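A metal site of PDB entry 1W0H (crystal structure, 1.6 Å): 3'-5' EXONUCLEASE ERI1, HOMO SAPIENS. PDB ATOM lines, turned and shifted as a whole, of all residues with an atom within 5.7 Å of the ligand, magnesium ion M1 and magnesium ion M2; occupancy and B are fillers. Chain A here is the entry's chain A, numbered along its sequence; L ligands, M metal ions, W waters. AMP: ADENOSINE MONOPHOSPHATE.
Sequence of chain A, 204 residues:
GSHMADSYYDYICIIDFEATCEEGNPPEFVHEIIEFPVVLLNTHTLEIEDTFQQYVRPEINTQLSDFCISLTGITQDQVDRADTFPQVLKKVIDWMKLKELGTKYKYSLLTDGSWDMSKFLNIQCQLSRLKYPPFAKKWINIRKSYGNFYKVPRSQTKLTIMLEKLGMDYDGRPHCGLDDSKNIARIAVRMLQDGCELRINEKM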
ATOM      1  N   ASP A  16      -2.935 -10.935  15.285  1.00  0.00           N
ATOM      2  CA  ASP A  16      -3.166 -11.235  13.889  1.00  0.00           C
ATOM      3  C   ASP A  16      -3.934 -10.054  13.281  1.00  0.00           C
ATOM      4  O   ASP A  16      -5.094  -9.839  13.599  1.00  0.00           O
ATOM      5  CB  ASP A  16      -3.970 -12.526  13.764  1.00  0.00           C
ATOM      6  CG  ASP A  16      -3.997 -13.000  12.385  1.00  0.00           C
ATOM      7  OD1 ASP A  16      -2.964 -13.544  11.913  1.00  0.00           O
ATOM      8  OD2 ASP A  16      -4.972 -12.779  11.627  1.00  0.00           O
ATOM      9  N   PHE A  17      -3.264  -9.282  12.437  1.00  0.00           N
ATOM     10  CA  PHE A  17      -3.848  -8.082  11.857  1.00  0.00           C
ATOM     11  C   PHE A  17      -4.799  -8.360  10.699  1.00  0.00           C
ATOM     12  O   PHE A  17      -4.688  -9.379   9.984  1.00  0.00           O
ATOM     13  CB  PHE A  17      -2.750  -7.143  11.327  1.00  0.00           C
ATOM     14  CG  PHE A  17      -1.810  -6.626  12.371  1.00  0.00           C
ATOM     15  CD1 PHE A  17      -2.271  -5.801  13.400  1.00  0.00           C
ATOM     16  CD2 PHE A  17      -0.440  -6.943  12.301  1.00  0.00           C
ATOM     17  CE1 PHE A  17      -1.373  -5.289  14.351  1.00  0.00           C
ATOM     18  CE2 PHE A  17       0.463  -6.457  13.261  1.00  0.00           C
ATOM     19  CZ  PHE A  17      -0.006  -5.642  14.287  1.00  0.00           C
ATOM     20  N   GLU A  18      -5.749  -7.436  10.512  1.00  0.00           N
ATOM     21  CA  GLU A  18      -6.345  -7.273   9.178  1.00  0.00           C
ATOM     22  C   GLU A  18      -5.825  -5.975   8.573  1.00  0.00           C
ATOM     23  O   GLU A  18      -5.484  -5.019   9.316  1.00  0.00           O
ATOM     24  CB  GLU A  18      -7.889  -7.247   9.189  1.00  0.00           C
ATOM     25  CG  GLU A  18      -8.534  -8.453   9.902  1.00  0.00           C
ATOM     26  CD  GLU A  18      -8.077  -9.782   9.340  1.00  0.00           C
ATOM     27  OE1 GLU A  18      -7.897  -9.922   8.101  1.00  0.00           O
ATOM     28  OE2 GLU A  18      -7.873 -10.735  10.158  1.00  0.00           O
ATOM     29  N   ALA A  19      -5.741  -5.965   7.252  1.00  0.00           N
ATOM     30  CA  ALA A  19      -5.224  -4.808   6.519  1.00  0.00           C
ATOM     31  C   ALA A  19      -6.065  -4.487   5.314  1.00  0.00           C
ATOM     32  O   ALA A  19      -6.801  -5.357   4.795  1.00  0.00           O
ATOM     33  CB  ALA A  19      -3.775  -5.073   6.067  1.00  0.00           C
ATOM     34  N   THR A  20      -5.968  -3.251   4.840  1.00  0.00           N
ATOM     35  CA  THR A  20      -6.558  -2.914   3.538  1.00  0.00           C
ATOM     36  C   THR A  20      -5.996  -3.838   2.457  1.00  0.00           C
ATOM     37  O   THR A  20      -4.859  -4.288   2.550  1.00  0.00           O
ATOM     38  CB  THR A  20      -6.265  -1.476   3.105  1.00  0.00           C
ATOM     39  OG1 THR A  20      -4.852  -1.243   3.123  1.00  0.00           O
ATOM     40  CG2 THR A  20      -6.892  -0.481   4.085  1.00  0.00           C
ATOM     41  N   CYS A  21      -6.800  -4.099   1.443  1.00  0.00           N
ATOM     42  CA  CYS A  21      -6.367  -4.981   0.362  1.00  0.00           C
ATOM     43  C   CYS A  21      -7.255  -4.745  -0.839  1.00  0.00           C
ATOM     44  O   CYS A  21      -8.309  -4.098  -0.739  1.00  0.00           O
ATOM     45  CB  CYS A  21      -6.403  -6.449   0.777  1.00  0.00           C
ATOM     46  SG  CYS A  21      -8.048  -6.983   1.380  1.00  0.00           S
ATOM     47  N   GLU A  22      -6.813  -5.282  -1.970  1.00  0.00           N
ATOM     48  CA  GLU A  22      -7.617  -5.318  -3.185  1.00  0.00           C
ATOM     49  C   GLU A  22      -7.641  -6.745  -3.719  1.00  0.00           C
ATOM     50  O   GLU A  22      -6.739  -7.561  -3.442  1.00  0.00           O
ATOM     51  CB  GLU A  22      -7.043  -4.379  -4.247  1.00  0.00           C
ATOM     52  CG  GLU A  22      -7.238  -2.921  -3.878  1.00  0.00           C
ATOM     53  CD  GLU A  22      -6.739  -1.954  -4.947  1.00  0.00           C
ATOM     54  OE1 GLU A  22      -5.830  -2.333  -5.711  1.00  0.00           O
ATOM     55  OE2 GLU A  22      -7.262  -0.815  -5.021  1.00  0.00           O
ATOM     56  N   GLU A  23      -8.694  -7.036  -4.465  1.00  0.00           N
ATOM     57  CA  GLU A  23      -8.833  -8.361  -5.055  1.00  0.00           C
ATOM     58  C   GLU A  23      -7.618  -8.648  -5.948  1.00  0.00           C
ATOM     59  O   GLU A  23      -7.200  -7.775  -6.710  1.00  0.00           O
ATOM     60  CB  GLU A  23     -10.115  -8.439  -5.885  1.00  0.00           C
ATOM     61  CG  GLU A  23     -10.461  -9.867  -6.302  1.00  0.00           C
ATOM     62  CD  GLU A  23     -11.868 -10.024  -6.843  1.00  0.00           C
ATOM     63  OE1 GLU A  23     -12.553  -9.013  -7.087  1.00  0.00           O
ATOM     64  OE2 GLU A  23     -12.289 -11.194  -7.021  1.00  0.00           O
ATOM     65  N   GLY A  24      -7.059  -9.843  -5.816  1.00  0.00           N
ATOM     66  CA  GLY A  24      -5.909 -10.223  -6.616  1.00  0.00           C
ATOM     67  C   GLY A  24      -4.564  -9.878  -5.992  1.00  0.00           C
ATOM     68  O   GLY A  24      -3.523 -10.233  -6.560  1.00  0.00           O
ATOM     69  N   ASN A  25      -4.589  -9.193  -4.842  1.00  0.00           N
ATOM     70  CA  ASN A  25      -3.356  -8.896  -4.117  1.00  0.00           C
ATOM     71  C   ASN A  25      -2.303  -8.179  -4.992  1.00  0.00           C
ATOM     72  O   ASN A  25      -1.139  -8.649  -5.113  1.00  0.00           O
ATOM     73  CB  ASN A  25      -2.803 -10.214  -3.528  1.00  0.00           C
ATOM     74  CG  ASN A  25      -1.617  -9.996  -2.618  1.00  0.00           C
ATOM     75  OD1 ASN A  25      -1.562  -9.038  -1.874  1.00  0.00           O
ATOM     76  ND2 ASN A  25      -0.656 -10.916  -2.676  1.00  0.00           N
ATOM     77  N   HIS A  31      -0.461  -1.705   1.751  1.00  0.00           N
ATOM     78  CA  HIS A  31      -1.293  -2.150   2.881  1.00  0.00           C
ATOM     79  C   HIS A  31      -1.243  -1.202   4.076  1.00  0.00           C
ATOM     80  O   HIS A  31      -0.158  -0.739   4.481  1.00  0.00           O
ATOM     81  CB  HIS A  31      -0.833  -3.504   3.405  1.00  0.00           C
ATOM     82  CG  HIS A  31      -1.014  -4.643   2.473  1.00  0.00           C
ATOM     83  ND1 HIS A  31      -2.260  -5.139   2.129  1.00  0.00           N
ATOM     84  CD2 HIS A  31      -0.110  -5.475   1.899  1.00  0.00           C
ATOM     85  CE1 HIS A  31      -2.109  -6.200   1.344  1.00  0.00           C
ATOM     86  NE2 HIS A  31      -0.816  -6.418   1.187  1.00  0.00           N
ATOM     87  N   PHE A  67     -13.914  -5.776  -1.949  1.00  0.00           N
ATOM     88  CA  PHE A  67     -13.263  -7.031  -1.640  1.00  0.00           C
ATOM     89  C   PHE A  67     -12.811  -7.078  -0.161  1.00  0.00           C
ATOM     90  O   PHE A  67     -13.037  -8.047   0.543  1.00  0.00           O
ATOM     91  CB  PHE A  67     -12.070  -7.291  -2.595  1.00  0.00           C
ATOM     92  CG  PHE A  67     -11.319  -8.526  -2.284  1.00  0.00           C
ATOM     93  CD1 PHE A  67     -11.738  -9.764  -2.793  1.00  0.00           C
ATOM     94  CD2 PHE A  67     -10.204  -8.476  -1.435  1.00  0.00           C
ATOM     95  CE1 PHE A  67     -11.040 -10.921  -2.471  1.00  0.00           C
ATOM     96  CE2 PHE A  67      -9.524  -9.640  -1.102  1.00  0.00           C
ATOM     97  CZ  PHE A  67      -9.938 -10.859  -1.625  1.00  0.00           C
ATOM     98  N   LEU A  71     -14.117  -9.653   2.597  1.00  0.00           N
ATOM     99  CA  LEU A  71     -13.176 -10.583   3.204  1.00  0.00           C
ATOM    100  C   LEU A  71     -13.179 -10.509   4.724  1.00  0.00           C
ATOM    101  O   LEU A  71     -13.327 -11.534   5.400  1.00  0.00           O
ATOM    102  CB  LEU A  71     -11.755 -10.320   2.657  1.00  0.00           C
ATOM    103  CG  LEU A  71     -10.645 -11.144   3.290  1.00  0.00           C
ATOM    104  CD1 LEU A  71     -10.711 -12.595   2.797  1.00  0.00           C
ATOM    105  CD2 LEU A  71      -9.278 -10.540   2.926  1.00  0.00           C
ATOM    106  N   THR A  72     -13.037  -9.303   5.260  1.00  0.00           N
ATOM    107  CA  THR A  72     -12.806  -9.103   6.680  1.00  0.00           C
ATOM    108  C   THR A  72     -14.061  -8.826   7.488  1.00  0.00           C
ATOM    109  O   THR A  72     -14.053  -8.968   8.711  1.00  0.00           O
ATOM    110  CB  THR A  72     -11.841  -7.898   6.935  1.00  0.00           C
ATOM    111  OG1 THR A  72     -12.498  -6.678   6.534  1.00  0.00           O
ATOM    112  CG2 THR A  72     -10.574  -7.989   6.063  1.00  0.00           C
ATOM    113  N   ASP A 112       0.571 -16.142  13.316  1.00  0.00           N
ATOM    114  CA  ASP A 112       0.256 -17.133  12.319  1.00  0.00           C
ATOM    115  C   ASP A 112       1.139 -17.032  11.061  1.00  0.00           C
ATOM    116  O   ASP A 112       0.697 -17.332   9.950  1.00  0.00           O
ATOM    117  CB  ASP A 112      -1.219 -16.929  11.961  1.00  0.00           C
ATOM    118  CG  ASP A 112      -1.749 -17.972  11.050  1.00  0.00           C
ATOM    119  OD1 ASP A 112      -1.249 -19.115  11.104  1.00  0.00           O
ATOM    120  OD2 ASP A 112      -2.662 -17.737  10.231  1.00  0.00           O
ATOM    121  N   ASP A 116       1.548 -12.101   8.814  1.00  0.00           N
ATOM    122  CA  ASP A 116       0.304 -11.835   9.527  1.00  0.00           C
ATOM    123  C   ASP A 116       0.415 -10.895  10.707  1.00  0.00           C
ATOM    124  O   ASP A 116      -0.585 -10.323  11.151  1.00  0.00           O
ATOM    125  CB  ASP A 116      -0.266 -13.182   9.987  1.00  0.00           C
ATOM    126  CG  ASP A 116      -0.756 -14.030   8.832  1.00  0.00           C
ATOM    127  OD1 ASP A 116       0.102 -14.416   7.975  1.00  0.00           O
ATOM    128  OD2 ASP A 116      -1.980 -14.322   8.695  1.00  0.00           O
ATOM    129  N   PHE A 120       2.990  -6.745   8.097  1.00  0.00           N
ATOM    130  CA  PHE A 120       2.006  -5.639   8.131  1.00  0.00           C
ATOM    131  C   PHE A 120       2.439  -4.535   9.077  1.00  0.00           C
ATOM    132  O   PHE A 120       2.295  -3.359   8.724  1.00  0.00           O
ATOM    133  CB  PHE A 120       0.582  -6.106   8.544  1.00  0.00           C
ATOM    134  CG  PHE A 120      -0.107  -6.927   7.473  1.00  0.00           C
ATOM    135  CD1 PHE A 120      -0.282  -6.438   6.179  1.00  0.00           C
ATOM    136  CD2 PHE A 120      -0.575  -8.203   7.778  1.00  0.00           C
ATOM    137  CE1 PHE A 120      -0.932  -7.190   5.186  1.00  0.00           C
ATOM    138  CE2 PHE A 120      -1.233  -8.966   6.781  1.00  0.00           C
ATOM    139  CZ  PHE A 120      -1.400  -8.457   5.495  1.00  0.00           C
ATOM    140  N   HIS A 175     -11.139 -14.161   9.213  1.00  0.00           N
ATOM    141  CA  HIS A 175     -10.699 -12.822   8.764  1.00  0.00           C
ATOM    142  C   HIS A 175     -11.257 -11.649   9.543  1.00  0.00           C
ATOM    143  O   HIS A 175     -11.055 -10.493   9.148  1.00  0.00           O
ATOM    144  CB  HIS A 175     -10.861 -12.638   7.245  1.00  0.00           C
ATOM    145  CG  HIS A 175     -10.414 -13.830   6.457  1.00  0.00           C
ATOM    146  ND1 HIS A 175      -9.082 -14.150   6.314  1.00  0.00           N
ATOM    147  CD2 HIS A 175     -11.115 -14.802   5.831  1.00  0.00           C
ATOM    148  CE1 HIS A 175      -8.982 -15.276   5.611  1.00  0.00           C
ATOM    149  NE2 HIS A 175     -10.207 -15.686   5.300  1.00  0.00           N
ATOM    150  N   CYS A 176     -11.980 -11.918  10.629  1.00  0.00           N
ATOM    151  CA  CYS A 176     -12.070 -10.982  11.746  1.00  0.00           C
ATOM    152  C   CYS A 176     -10.753 -11.169  12.509  1.00  0.00           C
ATOM    153  O   CYS A 176     -10.408 -12.291  12.913  1.00  0.00           O
ATOM    154  CB  CYS A 176     -13.274 -11.325  12.638  1.00  0.00           C
ATOM    155  SG  CYS A 176     -13.326 -10.562  14.259  1.00  0.00           S
ATOM    156  N   GLY A 177      -9.987 -10.094  12.711  1.00  0.00           N
ATOM    157  CA  GLY A 177      -8.681 -10.246  13.347  1.00  0.00           C
ATOM    158  C   GLY A 177      -8.744 -10.807  14.765  1.00  0.00           C
ATOM    159  O   GLY A 177      -7.909 -11.640  15.136  1.00  0.00           O
ATOM    160  N   ASP A 180      -9.646 -14.576  14.423  1.00  0.00           N
ATOM    161  CA  ASP A 180      -8.468 -15.348  14.000  1.00  0.00           C
ATOM    162  C   ASP A 180      -7.464 -15.466  15.141  1.00  0.00           C
ATOM    163  O   ASP A 180      -6.914 -16.538  15.363  1.00  0.00           O
ATOM    164  CB  ASP A 180      -7.749 -14.706  12.802  1.00  0.00           C
ATOM    165  CG  ASP A 180      -8.509 -14.820  11.500  1.00  0.00           C
ATOM    166  OD1 ASP A 180      -9.353 -15.715  11.325  1.00  0.00           O
ATOM    167  OD2 ASP A 180      -8.292 -14.041  10.559  1.00  0.00           O
ATOM    168  N   ILE A 184      -6.083 -18.926  16.803  1.00  0.00           N
ATOM    169  CA  ILE A 184      -4.667 -19.207  16.905  1.00  0.00           C
ATOM    170  C   ILE A 184      -4.309 -19.501  18.371  1.00  0.00           C
ATOM    171  O   ILE A 184      -3.541 -20.429  18.646  1.00  0.00           O
ATOM    172  CB  ILE A 184      -3.861 -18.000  16.349  1.00  0.00           C
ATOM    173  CG1 ILE A 184      -4.081 -17.893  14.841  1.00  0.00           C
ATOM    174  CG2 ILE A 184      -2.408 -18.211  16.597  1.00  0.00           C
ATOM    175  CD1 ILE A 184      -3.819 -16.478  14.281  1.00  0.00           C
HETATM  176  P   AMP L   1      -5.915 -12.908   7.270  1.00  0.00           P
HETATM  177  O1P AMP L   1      -5.170 -12.942   8.576  1.00  0.00           O
HETATM  178  O2P AMP L   1      -7.293 -12.272   7.461  1.00  0.00           O
HETATM  179  O3P AMP L   1      -6.110 -14.299   6.640  1.00  0.00           O
HETATM  180  O5' AMP L   1      -5.107 -12.035   6.189  1.00  0.00           O
HETATM  181  C5' AMP L   1      -4.566 -10.813   6.667  1.00  0.00           C
HETATM  182  C4' AMP L   1      -4.719  -9.766   5.560  1.00  0.00           C
HETATM  183  O4' AMP L   1      -4.106 -10.217   4.355  1.00  0.00           O
HETATM  184  C3' AMP L   1      -6.149  -9.384   5.138  1.00  0.00           C
HETATM  185  O3' AMP L   1      -6.696  -8.485   6.061  1.00  0.00           O
HETATM  186  C2' AMP L   1      -5.886  -8.838   3.752  1.00  0.00           C
HETATM  187  O2' AMP L   1      -5.328  -7.531   3.809  1.00  0.00           O
HETATM  188  C1' AMP L   1      -4.812  -9.794   3.224  1.00  0.00           C
HETATM  189  N9  AMP L   1      -5.473 -10.959   2.595  1.00  0.00           N
HETATM  190  C8  AMP L   1      -5.816 -12.151   3.202  1.00  0.00           C
HETATM  191  N7  AMP L   1      -6.393 -12.939   2.256  1.00  0.00           N
HETATM  192  C5  AMP L   1      -6.431 -12.260   1.087  1.00  0.00           C
HETATM  193  C6  AMP L   1      -6.905 -12.552  -0.193  1.00  0.00           C
HETATM  194  N6  AMP L   1      -7.478 -13.731  -0.457  1.00  0.00           N
HETATM  195  N1  AMP L   1      -6.779 -11.631  -1.199  1.00  0.00           N
HETATM  196  C2  AMP L   1      -6.200 -10.398  -0.978  1.00  0.00           C
HETATM  197  N3  AMP L   1      -5.739 -10.109   0.280  1.00  0.00           N
HETATM  198  C4  AMP L   1      -5.846 -11.008   1.292  1.00  0.00           C
HETATM  199 MG    MG M   1      -6.692 -12.530  10.227  1.00  0.00          MG
HETATM  200 MG    MG M   2      -3.599 -13.554   9.768  1.00  0.00          MG
HETATM  201  O   HOH W   1      -2.006 -12.992   5.469  1.00  0.00           O
HETATM  202  O   HOH W   2      -9.471 -14.558  -2.710  1.00  0.00           O
HETATM  203  O   HOH W   3      -7.466 -11.951  -3.859  1.00  0.00           O
HETATM  204  O   HOH W   4      -4.343 -15.606   9.940  1.00  0.00           O
HETATM  205  O   HOH W   5      -5.234 -15.189   4.482  1.00  0.00           O
HETATM  206  O   HOH W   6      -6.190 -16.427   8.237  1.00  0.00           O
HETATM  207  O   HOH W   7      -3.646  -8.381  -0.240  1.00  0.00           O
HETATM  208  O   HOH W   8      -7.923 -15.278   2.121  1.00  0.00           O
HETATM  209  O   HOH W   9      -2.946 -11.886   0.280  1.00  0.00           O
HETATM  210  O   HOH W  10      -2.882 -11.415   9.738  1.00  0.00           O
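The side-chain sulfur of Cys 21 sits close to an oxygen (O2') of the ligand (3.7 Å).
A ring nitrogen (ND1) of His 175 is in hydrogen-bond range of an oxygen (O2P) of the ligand, at 2.8 Å.
The backbone NH (N) of Ala 19 sits at hydrogen-bond distance from an oxygen (O3') of the ligand, at 2.9 Å.
The backbone carbonyl oxygen of Ala 19 is in hydrogen-bond range of an oxygen (O2') of the ligand, 2.8 Å away.
OD1 of Asp 180 is in hydrogen-bond range of N of His 175.
OE2 of Glu 18 lies close to N of Gly 177 (3.4 Å).
O of Thr 20 sits at hydrogen-bond distance from ND1 of His 31, 2.8 Å away.
O of Asp 116 is in hydrogen-bond range of N of Phe 17.
Merely in contact with the ligand: Phe 17 (3.6 Å), Thr 20 (3.5 Å), Glu 22 (3.8 Å), Phe 67 (3.3 Å), Leu 71 (3.8 Å), Thr 72 (3.9 Å) and Phe 120 (3.4 Å).
Hydrophobic or aromatic side chains within 4 Å of the ligand: Ala 19, Phe 67, Leu 71, Phe 120 and His 175.
The nearest printed residue that does not touch the ligand is His 31 (4.2 Å).
Merely in contact with magnesium ion M1: Phe 17.
Four residues have an atom within 4 Å of magnesium ion M1: Asp 16, Phe 17, Glu 18 and Asp 180.
Of the 22 residues printed, 2 come within 4 Å of magnesium ion M2.
Magnesium ion M1 is bound by OE2 of Glu 18, OD2 of Asp 180, OD2 of Asp 16 and O1P of the ligand.
Slightly farther from magnesium ion M1 lies an oxygen (O2P) of the ligand (2.8 Å).
Magnesium ion M2 is bound by an oxygen (O1P) of the ligand (2.1 Å), the side-chain carboxylate (OD2) of Asp 116 (2.1 Å), water W4 (2.2 Å), the side-chain carboxylate (OD1) of Asp 16 (2.2 Å), water W10 (2.3 Å) and the side-chain carboxylate (OD2) of Asp 16 (2.4 Å).
Water W10 bridges the backbone carbonyl oxygen (O) of Phe 17 and the backbone carbonyl oxygen (O) of Asp 116.
Water W7 bridges the side-chain amide oxygen (OD1) of Asn 25 and a nitrogen (N3) of the ligand.
Water W3 bridges a nitrogen (N1) of the ligand (2.8 Å) and the backbone NH of Gly 24 (2.9 Å).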
